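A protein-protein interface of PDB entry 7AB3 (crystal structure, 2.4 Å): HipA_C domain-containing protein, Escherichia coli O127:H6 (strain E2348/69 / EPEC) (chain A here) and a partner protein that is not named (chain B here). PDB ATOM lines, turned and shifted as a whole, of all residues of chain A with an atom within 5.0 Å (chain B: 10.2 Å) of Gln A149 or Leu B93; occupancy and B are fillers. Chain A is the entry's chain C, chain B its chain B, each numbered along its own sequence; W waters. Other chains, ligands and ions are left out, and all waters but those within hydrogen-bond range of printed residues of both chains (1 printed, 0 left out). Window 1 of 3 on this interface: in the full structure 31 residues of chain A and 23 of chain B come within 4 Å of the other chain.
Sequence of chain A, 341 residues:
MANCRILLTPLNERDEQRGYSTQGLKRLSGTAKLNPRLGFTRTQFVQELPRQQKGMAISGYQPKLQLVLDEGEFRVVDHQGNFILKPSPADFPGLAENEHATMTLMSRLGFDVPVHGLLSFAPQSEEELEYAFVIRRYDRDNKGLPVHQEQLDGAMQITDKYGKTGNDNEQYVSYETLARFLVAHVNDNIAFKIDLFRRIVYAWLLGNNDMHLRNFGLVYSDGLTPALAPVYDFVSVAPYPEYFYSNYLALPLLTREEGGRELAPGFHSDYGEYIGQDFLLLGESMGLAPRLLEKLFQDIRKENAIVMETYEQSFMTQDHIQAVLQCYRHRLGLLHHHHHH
Printed residues of chain A that touch a printed residue of chain B: Arg A137, Asp A139, Val A147, His A148, Gln A149, Glu A150, Gln A151, Leu A218 and Tyr A220. Of the 26 printed residues of chain B, 11 touch a printed residue of chain A. Printed residues of chain B that touch a printed residue of chain A: Leu B9, Tyr B10, Ile B37, Ser B38, Ile B39, Tyr B56, Ser B59, Leu B92, Leu B93, Gly B94 and Ala B95. Among the printed residues, no Asp or Glu carboxylate lies within 4 Å of a Lys or Arg side-chain nitrogen of the other chain.
Water W1 lies within hydrogen-bond range of the backbone carbonyl oxygen of Gln A151 (3.3 Å) and the side-chain hydroxyl of Ser B59 (3.3 Å).
Gln A149 touches just these residues of chain B: Leu B93 and Gly B94. Printed residues of chain A within 4 Å of Leu B93: Arg A137 (3.7 Å), Asp A139 (3.5 Å) and Gln A149 (3.3 Å). Printed residues of chain B within 4 Å of Glu A150: Ser B38, Ile B39 and Tyr B56. Of the printed residues of chain A, Tyr B56 touches His A148 and Glu A150. Of the printed residues of chain A, Tyr B10 touches His A148 and Tyr A220. Of the printed residues of chain A, Ser B38 touches Glu A150 (2.8 Å). The nearest residue of chain B that does not touch Gln A149 is Tyr B56 (4.6 Å). The nearest printed residue of chain A that does not touch Ile B39 is Gln A151 (7.1 Å).
N of Tyr B10 lies within hydrogen-bond range of O of Ala B95 (2.9 Å). The side-chain carboxylate (OD2) of Asp A139 lies within salt-bridge range of the guanidinium group (NH2) of Arg A137. The backbone carbonyl oxygen (O) of Asp A139 is in hydrogen-bond range of the backbone NH (N) of Val A147, 3.1 Å away. O of Ala B95 lies close to OE1 of Gln B97 (3.3 Å). OH of Tyr A138 is in hydrogen-bond range of OE1 of Gln A151, 3.5 Å away. N of Tyr A220 sits at hydrogen-bond distance from O of His A148, at 2.8 Å.
Leu B92 touches Arg A137 (O to NH2, 3.8 Å). Asp A139 touches Leu B93. Val A147 touches Gly B94. Leu B9 touches His A148 (CD1 to NE2, 3.5 Å). His A148 touches Ile B37 (CE1 to O, 2.9 Å). Leu B93 touches Gln A149. Gln A149 touches Gly B94 (N to CA, 3.9 Å). OG of Ser B59 touches CB of Gln A151, 3.9 Å away. Leu A218 touches Ile B39 (CD1 to CD1, 3.7 Å). Tyr A220 touches Tyr B10 (O to OH, 3.99 Å).
The side-chain hydroxyl (OH) of Tyr B10 lies close to the backbone NH (N) of His A148. The backbone NH (N) of Ile B39 is in hydrogen-bond range of the side-chain carboxylate (OE2) of Glu A150, at 2.9 Å. The side-chain hydroxyl (OG) of Ser B38 sits at hydrogen-bond distance from the side-chain carboxylate (OE1) of Glu A150 (2.8 Å). The backbone NH (N) of Gly B94 is in hydrogen-bond range of the side-chain carboxylate (OD2) of Asp A139 (2.9 Å). NE2 of His A148 is in hydrogen-bond range of OH of Tyr B56 (3.4 Å).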
ATOM      1  N   ARG A 137     -23.061 -10.015 -16.567  1.00  0.00           N
ATOM      2  CA  ARG A 137     -23.664  -8.972 -15.748  1.00  0.00           C
ATOM      3  C   ARG A 137     -25.164  -9.248 -15.571  1.00  0.00           C
ATOM      4  O   ARG A 137     -25.859  -9.521 -16.548  1.00  0.00           O
ATOM      5  CB  ARG A 137     -23.442  -7.590 -16.390  1.00  0.00           C
ATOM      6  CG  ARG A 137     -22.009  -7.099 -16.253  1.00  0.00           C
ATOM      7  CD  ARG A 137     -21.732  -5.814 -17.012  1.00  0.00           C
ATOM      8  NE  ARG A 137     -22.547  -4.699 -16.526  1.00  0.00           N
ATOM      9  CZ  ARG A 137     -22.208  -3.415 -16.628  1.00  0.00           C
ATOM     10  NH1 ARG A 137     -21.066  -3.065 -17.204  1.00  0.00           N
ATOM     11  NH2 ARG A 137     -23.016  -2.474 -16.166  1.00  0.00           N
ATOM     12  N   TYR A 138     -25.659  -9.201 -14.321  1.00  0.00           N
ATOM     13  CA  TYR A 138     -27.077  -9.427 -14.055  1.00  0.00           C
ATOM     14  C   TYR A 138     -27.953  -8.194 -14.360  1.00  0.00           C
ATOM     15  O   TYR A 138     -29.163  -8.332 -14.506  1.00  0.00           O
ATOM     16  CB  TYR A 138     -27.315  -9.955 -12.632  1.00  0.00           C
ATOM     17  CG  TYR A 138     -26.939  -8.997 -11.518  1.00  0.00           C
ATOM     18  CD1 TYR A 138     -27.796  -7.969 -11.137  1.00  0.00           C
ATOM     19  CD2 TYR A 138     -25.767  -9.166 -10.790  1.00  0.00           C
ATOM     20  CE1 TYR A 138     -27.452  -7.079 -10.127  1.00  0.00           C
ATOM     21  CE2 TYR A 138     -25.422  -8.298  -9.760  1.00  0.00           C
ATOM     22  CZ  TYR A 138     -26.275  -7.261  -9.425  1.00  0.00           C
ATOM     23  OH  TYR A 138     -25.961  -6.392  -8.412  1.00  0.00           O
ATOM     24  N   ASP A 139     -27.343  -6.994 -14.485  1.00  0.00           N
ATOM     25  CA  ASP A 139     -28.051  -5.754 -14.807  1.00  0.00           C
ATOM     26  C   ASP A 139     -28.275  -5.605 -16.315  1.00  0.00           C
ATOM     27  O   ASP A 139     -28.224  -4.500 -16.850  1.00  0.00           O
ATOM     28  CB  ASP A 139     -27.339  -4.520 -14.220  1.00  0.00           C
ATOM     29  CG  ASP A 139     -25.950  -4.259 -14.762  1.00  0.00           C
ATOM     30  OD1 ASP A 139     -25.247  -5.228 -15.074  1.00  0.00           O
ATOM     31  OD2 ASP A 139     -25.569  -3.081 -14.865  1.00  0.00           O
ATOM     32  N   VAL A 147     -30.970  -3.143 -16.908  1.00  0.00           N
ATOM     33  CA  VAL A 147     -31.963  -3.390 -15.875  1.00  0.00           C
ATOM     34  C   VAL A 147     -31.470  -2.634 -14.665  1.00  0.00           C
ATOM     35  O   VAL A 147     -30.298  -2.778 -14.304  1.00  0.00           O
ATOM     36  CB  VAL A 147     -32.111  -4.887 -15.556  1.00  0.00           C
ATOM     37  CG1 VAL A 147     -33.133  -5.095 -14.447  1.00  0.00           C
ATOM     38  CG2 VAL A 147     -32.506  -5.664 -16.801  1.00  0.00           C
ATOM     39  N   HIS A 148     -32.330  -1.791 -14.061  1.00  0.00           N
ATOM     40  CA  HIS A 148     -31.890  -0.989 -12.926  1.00  0.00           C
ATOM     41  C   HIS A 148     -31.667  -1.801 -11.655  1.00  0.00           C
ATOM     42  O   HIS A 148     -32.331  -2.799 -11.413  1.00  0.00           O
ATOM     43  CB  HIS A 148     -32.788   0.213 -12.668  1.00  0.00           C
ATOM     44  CG  HIS A 148     -32.167   1.205 -11.735  1.00  0.00           C
ATOM     45  ND1 HIS A 148     -32.839   1.638 -10.613  1.00  0.00           N
ATOM     46  CD2 HIS A 148     -30.939   1.785 -11.764  1.00  0.00           C
ATOM     47  CE1 HIS A 148     -32.018   2.473 -10.007  1.00  0.00           C
ATOM     48  NE2 HIS A 148     -30.866   2.604 -10.663  1.00  0.00           N
ATOM     49  N   GLN A 149     -30.652  -1.406 -10.901  1.00  0.00           N
ATOM     50  CA  GLN A 149     -30.263  -2.053  -9.684  1.00  0.00           C
ATOM     51  C   GLN A 149     -29.550  -1.083  -8.746  1.00  0.00           C
ATOM     52  O   GLN A 149     -29.114   0.001  -9.158  1.00  0.00           O
ATOM     53  CB  GLN A 149     -29.379  -3.280  -9.996  1.00  0.00           C
ATOM     54  CG  GLN A 149     -27.974  -2.959 -10.514  1.00  0.00           C
ATOM     55  CD  GLN A 149     -26.919  -3.021  -9.434  1.00  0.00           C
ATOM     56  OE1 GLN A 149     -26.086  -2.124  -9.296  1.00  0.00           O
ATOM     57  NE2 GLN A 149     -26.947  -4.064  -8.613  1.00  0.00           N
ATOM     58  N   GLU A 150     -29.435  -1.471  -7.473  1.00  0.00           N
ATOM     59  CA  GLU A 150     -28.693  -0.682  -6.511  1.00  0.00           C
ATOM     60  C   GLU A 150     -28.077  -1.544  -5.417  1.00  0.00           C
ATOM     61  O   GLU A 150     -28.613  -2.600  -5.092  1.00  0.00           O
ATOM     62  CB  GLU A 150     -29.526   0.469  -5.954  1.00  0.00           C
ATOM     63  CG  GLU A 150     -30.602   0.020  -4.996  1.00  0.00           C
ATOM     64  CD  GLU A 150     -31.234   1.182  -4.273  1.00  0.00           C
ATOM     65  OE1 GLU A 150     -30.507   2.154  -3.959  1.00  0.00           O
ATOM     66  OE2 GLU A 150     -32.458   1.117  -4.025  1.00  0.00           O
ATOM     67  N   GLN A 151     -26.939  -1.111  -4.866  1.00  0.00           N
ATOM     68  CA  GLN A 151     -26.284  -1.858  -3.784  1.00  0.00           C
ATOM     69  C   GLN A 151     -26.929  -1.531  -2.445  1.00  0.00           C
ATOM     70  O   GLN A 151     -27.468  -0.443  -2.272  1.00  0.00           O
ATOM     71  CB  GLN A 151     -24.768  -1.607  -3.758  1.00  0.00           C
ATOM     72  CG  GLN A 151     -23.955  -2.712  -4.391  1.00  0.00           C
ATOM     73  CD  GLN A 151     -24.307  -2.922  -5.826  1.00  0.00           C
ATOM     74  OE1 GLN A 151     -24.784  -3.984  -6.229  1.00  0.00           O
ATOM     75  NE2 GLN A 151     -24.051  -1.910  -6.635  1.00  0.00           N
ATOM     76  N   GLY A 217     -27.444  -6.736  -3.553  1.00  0.00           N
ATOM     77  CA  GLY A 217     -28.073  -5.784  -4.453  1.00  0.00           C
ATOM     78  C   GLY A 217     -29.562  -5.971  -4.554  1.00  0.00           C
ATOM     79  O   GLY A 217     -30.109  -6.975  -4.097  1.00  0.00           O
ATOM     80  N   LEU A 218     -30.219  -5.004  -5.171  1.00  0.00           N
ATOM     81  CA  LEU A 218     -31.649  -5.064  -5.446  1.00  0.00           C
ATOM     82  C   LEU A 218     -31.843  -4.877  -6.932  1.00  0.00           C
ATOM     83  O   LEU A 218     -31.398  -3.870  -7.460  1.00  0.00           O
ATOM     84  CB  LEU A 218     -32.405  -3.958  -4.699  1.00  0.00           C
ATOM     85  CG  LEU A 218     -32.409  -4.094  -3.198  1.00  0.00           C
ATOM     86  CD1 LEU A 218     -33.108  -2.920  -2.572  1.00  0.00           C
ATOM     87  CD2 LEU A 218     -33.057  -5.422  -2.770  1.00  0.00           C
ATOM     88  N   VAL A 219     -32.487  -5.829  -7.611  1.00  0.00           N
ATOM     89  CA  VAL A 219     -32.759  -5.691  -9.040  1.00  0.00           C
ATOM     90  C   VAL A 219     -34.198  -5.229  -9.279  1.00  0.00           C
ATOM     91  O   VAL A 219     -35.124  -5.685  -8.608  1.00  0.00           O
ATOM     92  CB  VAL A 219     -32.401  -6.955  -9.852  1.00  0.00           C
ATOM     93  CG1 VAL A 219     -32.518  -6.684 -11.343  1.00  0.00           C
ATOM     94  CG2 VAL A 219     -30.998  -7.408  -9.530  1.00  0.00           C
ATOM     95  N   TYR A 220     -34.372  -4.276 -10.188  1.00  0.00           N
ATOM     96  CA  TYR A 220     -35.684  -3.740 -10.539  1.00  0.00           C
ATOM     97  C   TYR A 220     -36.184  -4.350 -11.840  1.00  0.00           C
ATOM     98  O   TYR A 220     -36.080  -3.759 -12.921  1.00  0.00           O
ATOM     99  CB  TYR A 220     -35.725  -2.204 -10.530  1.00  0.00           C
ATOM    100  CG  TYR A 220     -35.353  -1.634  -9.179  1.00  0.00           C
ATOM    101  CD1 TYR A 220     -36.301  -1.487  -8.180  1.00  0.00           C
ATOM    102  CD2 TYR A 220     -34.043  -1.276  -8.889  1.00  0.00           C
ATOM    103  CE1 TYR A 220     -35.962  -0.965  -6.936  1.00  0.00           C
ATOM    104  CE2 TYR A 220     -33.692  -0.758  -7.652  1.00  0.00           C
ATOM    105  CZ  TYR A 220     -34.650  -0.622  -6.668  1.00  0.00           C
ATOM    106  OH  TYR A 220     -34.300  -0.122  -5.434  1.00  0.00           O
ATOM    107  N   LEU B   8     -29.682  10.870 -14.820  1.00  0.00           N
ATOM    108  CA  LEU B   8     -30.502  10.174 -15.810  1.00  0.00           C
ATOM    109  C   LEU B   8     -30.826   8.739 -15.400  1.00  0.00           C
ATOM    110  O   LEU B   8     -29.943   8.005 -14.973  1.00  0.00           O
ATOM    111  CB  LEU B   8     -29.779  10.130 -17.164  1.00  0.00           C
ATOM    112  CG  LEU B   8     -29.927  11.320 -18.095  1.00  0.00           C
ATOM    113  CD1 LEU B   8     -29.070  12.486 -17.634  1.00  0.00           C
ATOM    114  CD2 LEU B   8     -29.529  10.936 -19.507  1.00  0.00           C
ATOM    115  N   LEU B   9     -32.082   8.324 -15.570  1.00  0.00           N
ATOM    116  CA  LEU B   9     -32.487   6.949 -15.304  1.00  0.00           C
ATOM    117  C   LEU B   9     -33.214   6.439 -16.540  1.00  0.00           C
ATOM    118  O   LEU B   9     -34.183   7.060 -16.985  1.00  0.00           O
ATOM    119  CB  LEU B   9     -33.373   6.817 -14.055  1.00  0.00           C
ATOM    120  CG  LEU B   9     -33.620   5.381 -13.562  1.00  0.00           C
ATOM    121  CD1 LEU B   9     -32.380   4.812 -12.885  1.00  0.00           C
ATOM    122  CD2 LEU B   9     -34.801   5.324 -12.617  1.00  0.00           C
ATOM    123  N   TYR B  10     -32.696   5.350 -17.128  1.00  0.00           N
ATOM    124  CA  TYR B  10     -33.231   4.708 -18.332  1.00  0.00           C
ATOM    125  C   TYR B  10     -33.054   5.568 -19.596  1.00  0.00           C
ATOM    126  O   TYR B  10     -33.850   5.457 -20.520  1.00  0.00           O
ATOM    127  CB  TYR B  10     -34.700   4.254 -18.148  1.00  0.00           C
ATOM    128  CG  TYR B  10     -34.866   3.028 -17.272  1.00  0.00           C
ATOM    129  CD1 TYR B  10     -34.418   1.782 -17.692  1.00  0.00           C
ATOM    130  CD2 TYR B  10     -35.514   3.106 -16.045  1.00  0.00           C
ATOM    131  CE1 TYR B  10     -34.575   0.651 -16.895  1.00  0.00           C
ATOM    132  CE2 TYR B  10     -35.669   1.984 -15.237  1.00  0.00           C
ATOM    133  CZ  TYR B  10     -35.202   0.756 -15.666  1.00  0.00           C
ATOM    134  OH  TYR B  10     -35.370  -0.359 -14.879  1.00  0.00           O
ATOM    135  N   PRO B  35     -40.232   5.758 -11.812  1.00  0.00           N
ATOM    136  CA  PRO B  35     -39.651   5.043 -10.662  1.00  0.00           C
ATOM    137  C   PRO B  35     -38.475   5.775 -10.015  1.00  0.00           C
ATOM    138  O   PRO B  35     -37.715   6.466 -10.693  1.00  0.00           O
ATOM    139  CB  PRO B  35     -39.230   3.695 -11.260  1.00  0.00           C
ATOM    140  CG  PRO B  35     -38.920   4.001 -12.685  1.00  0.00           C
ATOM    141  CD  PRO B  35     -39.792   5.182 -13.097  1.00  0.00           C
ATOM    142  N   ALA B  36     -38.325   5.615  -8.698  1.00  0.00           N
ATOM    143  CA  ALA B  36     -37.236   6.222  -7.940  1.00  0.00           C
ATOM    144  C   ALA B  36     -35.878   5.602  -8.326  1.00  0.00           C
ATOM    145  O   ALA B  36     -35.806   4.404  -8.603  1.00  0.00           O
ATOM    146  CB  ALA B  36     -37.486   6.037  -6.450  1.00  0.00           C
ATOM    147  N   ILE B  37     -34.805   6.416  -8.352  1.00  0.00           N
ATOM    148  CA  ILE B  37     -33.460   5.909  -8.651  1.00  0.00           C
ATOM    149  C   ILE B  37     -32.911   5.032  -7.497  1.00  0.00           C
ATOM    150  O   ILE B  37     -32.041   4.194  -7.714  1.00  0.00           O
ATOM    151  CB  ILE B  37     -32.485   7.056  -9.017  1.00  0.00           C
ATOM    152  CG1 ILE B  37     -32.262   8.012  -7.833  1.00  0.00           C
ATOM    153  CG2 ILE B  37     -32.966   7.803 -10.252  1.00  0.00           C
ATOM    154  CD1 ILE B  37     -31.179   9.012  -8.050  1.00  0.00           C
ATOM    155  N   SER B  38     -33.431   5.215  -6.281  1.00  0.00           N
ATOM    156  CA  SER B  38     -33.017   4.478  -5.105  1.00  0.00           C
ATOM    157  C   SER B  38     -34.179   4.393  -4.122  1.00  0.00           C
ATOM    158  O   SER B  38     -35.005   5.306  -4.079  1.00  0.00           O
ATOM    159  CB  SER B  38     -31.861   5.220  -4.441  1.00  0.00           C
ATOM    160  OG  SER B  38     -31.488   4.656  -3.195  1.00  0.00           O
ATOM    161  N   ILE B  39     -34.221   3.338  -3.283  1.00  0.00           N
ATOM    162  CA  ILE B  39     -35.253   3.271  -2.242  1.00  0.00           C
ATOM    163  C   ILE B  39     -34.991   4.341  -1.140  1.00  0.00           C
ATOM    164  O   ILE B  39     -35.915   4.720  -0.426  1.00  0.00           O
ATOM    165  CB  ILE B  39     -35.496   1.850  -1.690  1.00  0.00           C
ATOM    166  CG1 ILE B  39     -34.232   1.237  -1.110  1.00  0.00           C
ATOM    167  CG2 ILE B  39     -36.128   0.959  -2.764  1.00  0.00           C
ATOM    168  CD1 ILE B  39     -34.412  -0.130  -0.589  1.00  0.00           C
ATOM    169  N   TYR B  56     -26.446   7.060  -1.685  1.00  0.00           N
ATOM    170  CA  TYR B  56     -26.685   6.461  -2.990  1.00  0.00           C
ATOM    171  C   TYR B  56     -25.624   6.907  -3.992  1.00  0.00           C
ATOM    172  O   TYR B  56     -25.069   6.074  -4.701  1.00  0.00           O
ATOM    173  CB  TYR B  56     -28.088   6.800  -3.512  1.00  0.00           C
ATOM    174  CG  TYR B  56     -28.347   6.206  -4.877  1.00  0.00           C
ATOM    175  CD1 TYR B  56     -28.430   4.832  -5.052  1.00  0.00           C
ATOM    176  CD2 TYR B  56     -28.442   7.013  -6.004  1.00  0.00           C
ATOM    177  CE1 TYR B  56     -28.634   4.273  -6.306  1.00  0.00           C
ATOM    178  CE2 TYR B  56     -28.626   6.465  -7.269  1.00  0.00           C
ATOM    179  CZ  TYR B  56     -28.723   5.090  -7.414  1.00  0.00           C
ATOM    180  OH  TYR B  56     -28.925   4.526  -8.648  1.00  0.00           O
ATOM    181  N   SER B  59     -22.146   5.557  -3.068  1.00  0.00           N
ATOM    182  CA  SER B  59     -22.100   4.120  -3.388  1.00  0.00           C
ATOM    183  C   SER B  59     -21.885   3.859  -4.896  1.00  0.00           C
ATOM    184  O   SER B  59     -21.444   2.774  -5.272  1.00  0.00           O
ATOM    185  CB  SER B  59     -23.377   3.423  -2.912  1.00  0.00           C
ATOM    186  OG  SER B  59     -23.587   2.131  -3.464  1.00  0.00           O
ATOM    187  N   LEU B  60     -22.236   4.820  -5.748  1.00  0.00           N
ATOM    188  CA  LEU B  60     -22.075   4.731  -7.194  1.00  0.00           C
ATOM    189  C   LEU B  60     -20.599   4.840  -7.591  1.00  0.00           C
ATOM    190  O   LEU B  60     -20.186   4.232  -8.578  1.00  0.00           O
ATOM    191  CB  LEU B  60     -22.869   5.878  -7.826  1.00  0.00           C
ATOM    192  CG  LEU B  60     -24.152   5.551  -8.572  1.00  0.00           C
ATOM    193  CD1 LEU B  60     -25.047   4.611  -7.785  1.00  0.00           C
ATOM    194  CD2 LEU B  60     -24.893   6.821  -8.912  1.00  0.00           C
ATOM    195  N   ALA B  61     -19.802   5.612  -6.817  1.00  0.00           N
ATOM    196  CA  ALA B  61     -18.363   5.796  -7.047  1.00  0.00           C
ATOM    197  C   ALA B  61     -17.594   4.476  -6.861  1.00  0.00           C
ATOM    198  O   ALA B  61     -18.046   3.598  -6.122  1.00  0.00           O
ATOM    199  CB  ALA B  61     -17.821   6.846  -6.088  1.00  0.00           C
ATOM    200  N   PRO B  62     -16.423   4.305  -7.512  1.00  0.00           N
ATOM    201  CA  PRO B  62     -15.673   3.046  -7.322  1.00  0.00           C
ATOM    202  C   PRO B  62     -14.939   2.979  -5.971  1.00  0.00           C
ATOM    203  O   PRO B  62     -15.077   3.902  -5.152  1.00  0.00           O
ATOM    204  CB  PRO B  62     -14.760   2.979  -8.557  1.00  0.00           C
ATOM    205  CG  PRO B  62     -14.689   4.389  -9.097  1.00  0.00           C
ATOM    206  CD  PRO B  62     -15.706   5.248  -8.395  1.00  0.00           C
ATOM    207  N   LEU B  66     -10.440  -0.206  -9.723  1.00  0.00           N
ATOM    208  CA  LEU B  66     -10.956   0.669 -10.781  1.00  0.00           C
ATOM    209  C   LEU B  66     -10.889   2.156 -10.411  1.00  0.00           C
ATOM    210  O   LEU B  66     -10.693   3.001 -11.286  1.00  0.00           O
ATOM    211  CB  LEU B  66     -12.379   0.257 -11.236  1.00  0.00           C
ATOM    212  CG  LEU B  66     -12.528  -1.097 -11.976  1.00  0.00           C
ATOM    213  CD1 LEU B  66     -13.977  -1.366 -12.345  1.00  0.00           C
ATOM    214  CD2 LEU B  66     -11.690  -1.139 -13.221  1.00  0.00           C
ATOM    215  N   LEU B  85     -17.673  11.020  -9.751  1.00  0.00           N
ATOM    216  CA  LEU B  85     -18.896  10.391 -10.226  1.00  0.00           C
ATOM    217  C   LEU B  85     -19.271  10.855 -11.642  1.00  0.00           C
ATOM    218  O   LEU B  85     -19.859  10.088 -12.402  1.00  0.00           O
ATOM    219  CB  LEU B  85     -20.025  10.698  -9.222  1.00  0.00           C
ATOM    220  CG  LEU B  85     -21.384  10.037  -9.430  1.00  0.00           C
ATOM    221  CD1 LEU B  85     -21.260   8.536  -9.622  1.00  0.00           C
ATOM    222  CD2 LEU B  85     -22.302  10.341  -8.273  1.00  0.00           C
ATOM    223  N   ASN B  88     -17.133   8.958 -14.336  1.00  0.00           N
ATOM    224  CA  ASN B  88     -17.590   7.585 -14.579  1.00  0.00           C
ATOM    225  C   ASN B  88     -19.125   7.524 -14.686  1.00  0.00           C
ATOM    226  O   ASN B  88     -19.722   6.521 -14.318  1.00  0.00           O
ATOM    227  CB  ASN B  88     -17.116   6.637 -13.460  1.00  0.00           C
ATOM    228  CG  ASN B  88     -15.822   7.022 -12.770  1.00  0.00           C
ATOM    229  OD1 ASN B  88     -14.886   7.567 -13.373  1.00  0.00           O
ATOM    230  ND2 ASN B  88     -15.754   6.760 -11.478  1.00  0.00           N
ATOM    231  N   GLY B  89     -19.739   8.595 -15.183  1.00  0.00           N
ATOM    232  CA  GLY B  89     -21.183   8.735 -15.311  1.00  0.00           C
ATOM    233  C   GLY B  89     -21.809   7.879 -16.388  1.00  0.00           C
ATOM    234  O   GLY B  89     -22.899   7.339 -16.186  1.00  0.00           O
ATOM    235  N   LYS B  90     -21.145   7.761 -17.547  1.00  0.00           N
ATOM    236  CA  LYS B  90     -21.650   6.887 -18.609  1.00  0.00           C
ATOM    237  C   LYS B  90     -21.221   5.413 -18.410  1.00  0.00           C
ATOM    238  O   LYS B  90     -21.454   4.598 -19.297  1.00  0.00           O
ATOM    239  CB  LYS B  90     -21.256   7.405 -20.005  1.00  0.00           C
ATOM    240  CG  LYS B  90     -22.007   8.668 -20.422  1.00  0.00           C
ATOM    241  CD  LYS B  90     -21.720   9.063 -21.867  1.00  0.00           C
ATOM    242  CE  LYS B  90     -22.434  10.343 -22.256  1.00  0.00           C
ATOM    243  NZ  LYS B  90     -22.340  10.635 -23.716  1.00  0.00           N
ATOM    244  N   ASN B  91     -20.597   5.076 -17.261  1.00  0.00           N
ATOM    245  CA  ASN B  91     -20.155   3.725 -16.958  1.00  0.00           C
ATOM    246  C   ASN B  91     -20.553   3.331 -15.537  1.00  0.00           C
ATOM    247  O   ASN B  91     -19.701   3.071 -14.690  1.00  0.00           O
ATOM    248  CB  ASN B  91     -18.650   3.573 -17.178  1.00  0.00           C
ATOM    249  CG  ASN B  91     -18.171   2.138 -17.340  1.00  0.00           C
ATOM    250  OD1 ASN B  91     -16.967   1.869 -17.345  1.00  0.00           O
ATOM    251  ND2 ASN B  91     -19.083   1.169 -17.500  1.00  0.00           N
ATOM    252  N   LEU B  92     -21.858   3.282 -15.282  1.00  0.00           N
ATOM    253  CA  LEU B  92     -22.390   2.925 -13.973  1.00  0.00           C
ATOM    254  C   LEU B  92     -23.195   1.609 -14.022  1.00  0.00           C
ATOM    255  O   LEU B  92     -23.584   1.153 -15.101  1.00  0.00           O
ATOM    256  CB  LEU B  92     -23.279   4.078 -13.459  1.00  0.00           C
ATOM    257  CG  LEU B  92     -22.561   5.362 -13.083  1.00  0.00           C
ATOM    258  CD1 LEU B  92     -23.547   6.465 -12.806  1.00  0.00           C
ATOM    259  CD2 LEU B  92     -21.678   5.152 -11.881  1.00  0.00           C
ATOM    260  N   LEU B  93     -23.442   0.997 -12.851  1.00  0.00           N
ATOM    261  CA  LEU B  93     -24.244  -0.223 -12.793  1.00  0.00           C
ATOM    262  C   LEU B  93     -25.730   0.140 -12.811  1.00  0.00           C
ATOM    263  O   LEU B  93     -26.147   1.142 -12.220  1.00  0.00           O
ATOM    264  CB  LEU B  93     -23.924  -1.048 -11.543  1.00  0.00           C
ATOM    265  CG  LEU B  93     -22.711  -1.963 -11.604  1.00  0.00           C
ATOM    266  CD1 LEU B  93     -22.405  -2.517 -10.242  1.00  0.00           C
ATOM    267  CD2 LEU B  93     -22.944  -3.100 -12.554  1.00  0.00           C
ATOM    268  N   GLY B  94     -26.508  -0.692 -13.478  1.00  0.00           N
ATOM    269  CA  GLY B  94     -27.935  -0.479 -13.601  1.00  0.00           C
ATOM    270  C   GLY B  94     -28.293   0.401 -14.782  1.00  0.00           C
ATOM    271  O   GLY B  94     -27.675   0.317 -15.852  1.00  0.00           O
ATOM    272  N   ALA B  95     -29.315   1.247 -14.585  1.00  0.00           N
ATOM    273  CA  ALA B  95     -29.805   2.166 -15.600  1.00  0.00           C
ATOM    274  C   ALA B  95     -29.555   3.636 -15.250  1.00  0.00           C
ATOM    275  O   ALA B  95     -30.187   4.505 -15.832  1.00  0.00           O
ATOM    276  CB  ALA B  95     -31.285   1.929 -15.838  1.00  0.00           C
ATOM    277  N   ILE B  96     -28.620   3.920 -14.335  1.00  0.00           N
ATOM    278  CA  ILE B  96     -28.290   5.282 -13.925  1.00  0.00           C
ATOM    279  C   ILE B  96     -27.111   5.842 -14.751  1.00  0.00           C
ATOM    280  O   ILE B  96     -26.188   5.105 -15.117  1.00  0.00           O
ATOM    281  CB  ILE B  96     -28.031   5.336 -12.388  1.00  0.00           C
ATOM    282  CG1 ILE B  96     -28.130   6.762 -11.829  1.00  0.00           C
ATOM    283  CG2 ILE B  96     -26.715   4.657 -11.987  1.00  0.00           C
ATOM    284  CD1 ILE B  96     -29.480   7.166 -11.558  1.00  0.00           C
ATOM    285  N   GLN B  97     -27.189   7.141 -15.101  1.00  0.00           N
ATOM    286  CA  GLN B  97     -26.165   7.880 -15.849  1.00  0.00           C
ATOM    287  C   GLN B  97     -26.005   9.248 -15.190  1.00  0.00           C
ATOM    288  O   GLN B  97     -27.000   9.900 -14.919  1.00  0.00           O
ATOM    289  CB  GLN B  97     -26.572   8.083 -17.322  1.00  0.00           C
ATOM    290  CG  GLN B  97     -26.776   6.796 -18.117  1.00  0.00           C
ATOM    291  CD  GLN B  97     -28.100   6.813 -18.855  1.00  0.00           C
ATOM    292  OE1 GLN B  97     -29.082   6.166 -18.454  1.00  0.00           O
ATOM    293  NE2 GLN B  97     -28.158   7.568 -19.944  1.00  0.00           N
ATOM    294  N   ILE B  98     -24.771   9.680 -14.915  1.00  0.00           N
ATOM    295  CA  ILE B  98     -24.512  10.996 -14.324  1.00  0.00           C
ATOM    296  C   ILE B  98     -23.784  11.858 -15.355  1.00  0.00           C
ATOM    297  O   ILE B  98     -22.625  11.605 -15.675  1.00  0.00           O
ATOM    298  CB  ILE B  98     -23.736  10.889 -12.988  1.00  0.00           C
ATOM    299  CG1 ILE B  98     -24.473   9.980 -11.984  1.00  0.00           C
ATOM    300  CG2 ILE B  98     -23.464  12.269 -12.397  1.00  0.00           C
ATOM    301  CD1 ILE B  98     -25.850  10.435 -11.619  1.00  0.00           C
HETATM  302  O   HOH W   1     -26.870   2.310  -3.915  1.00  0.00           O
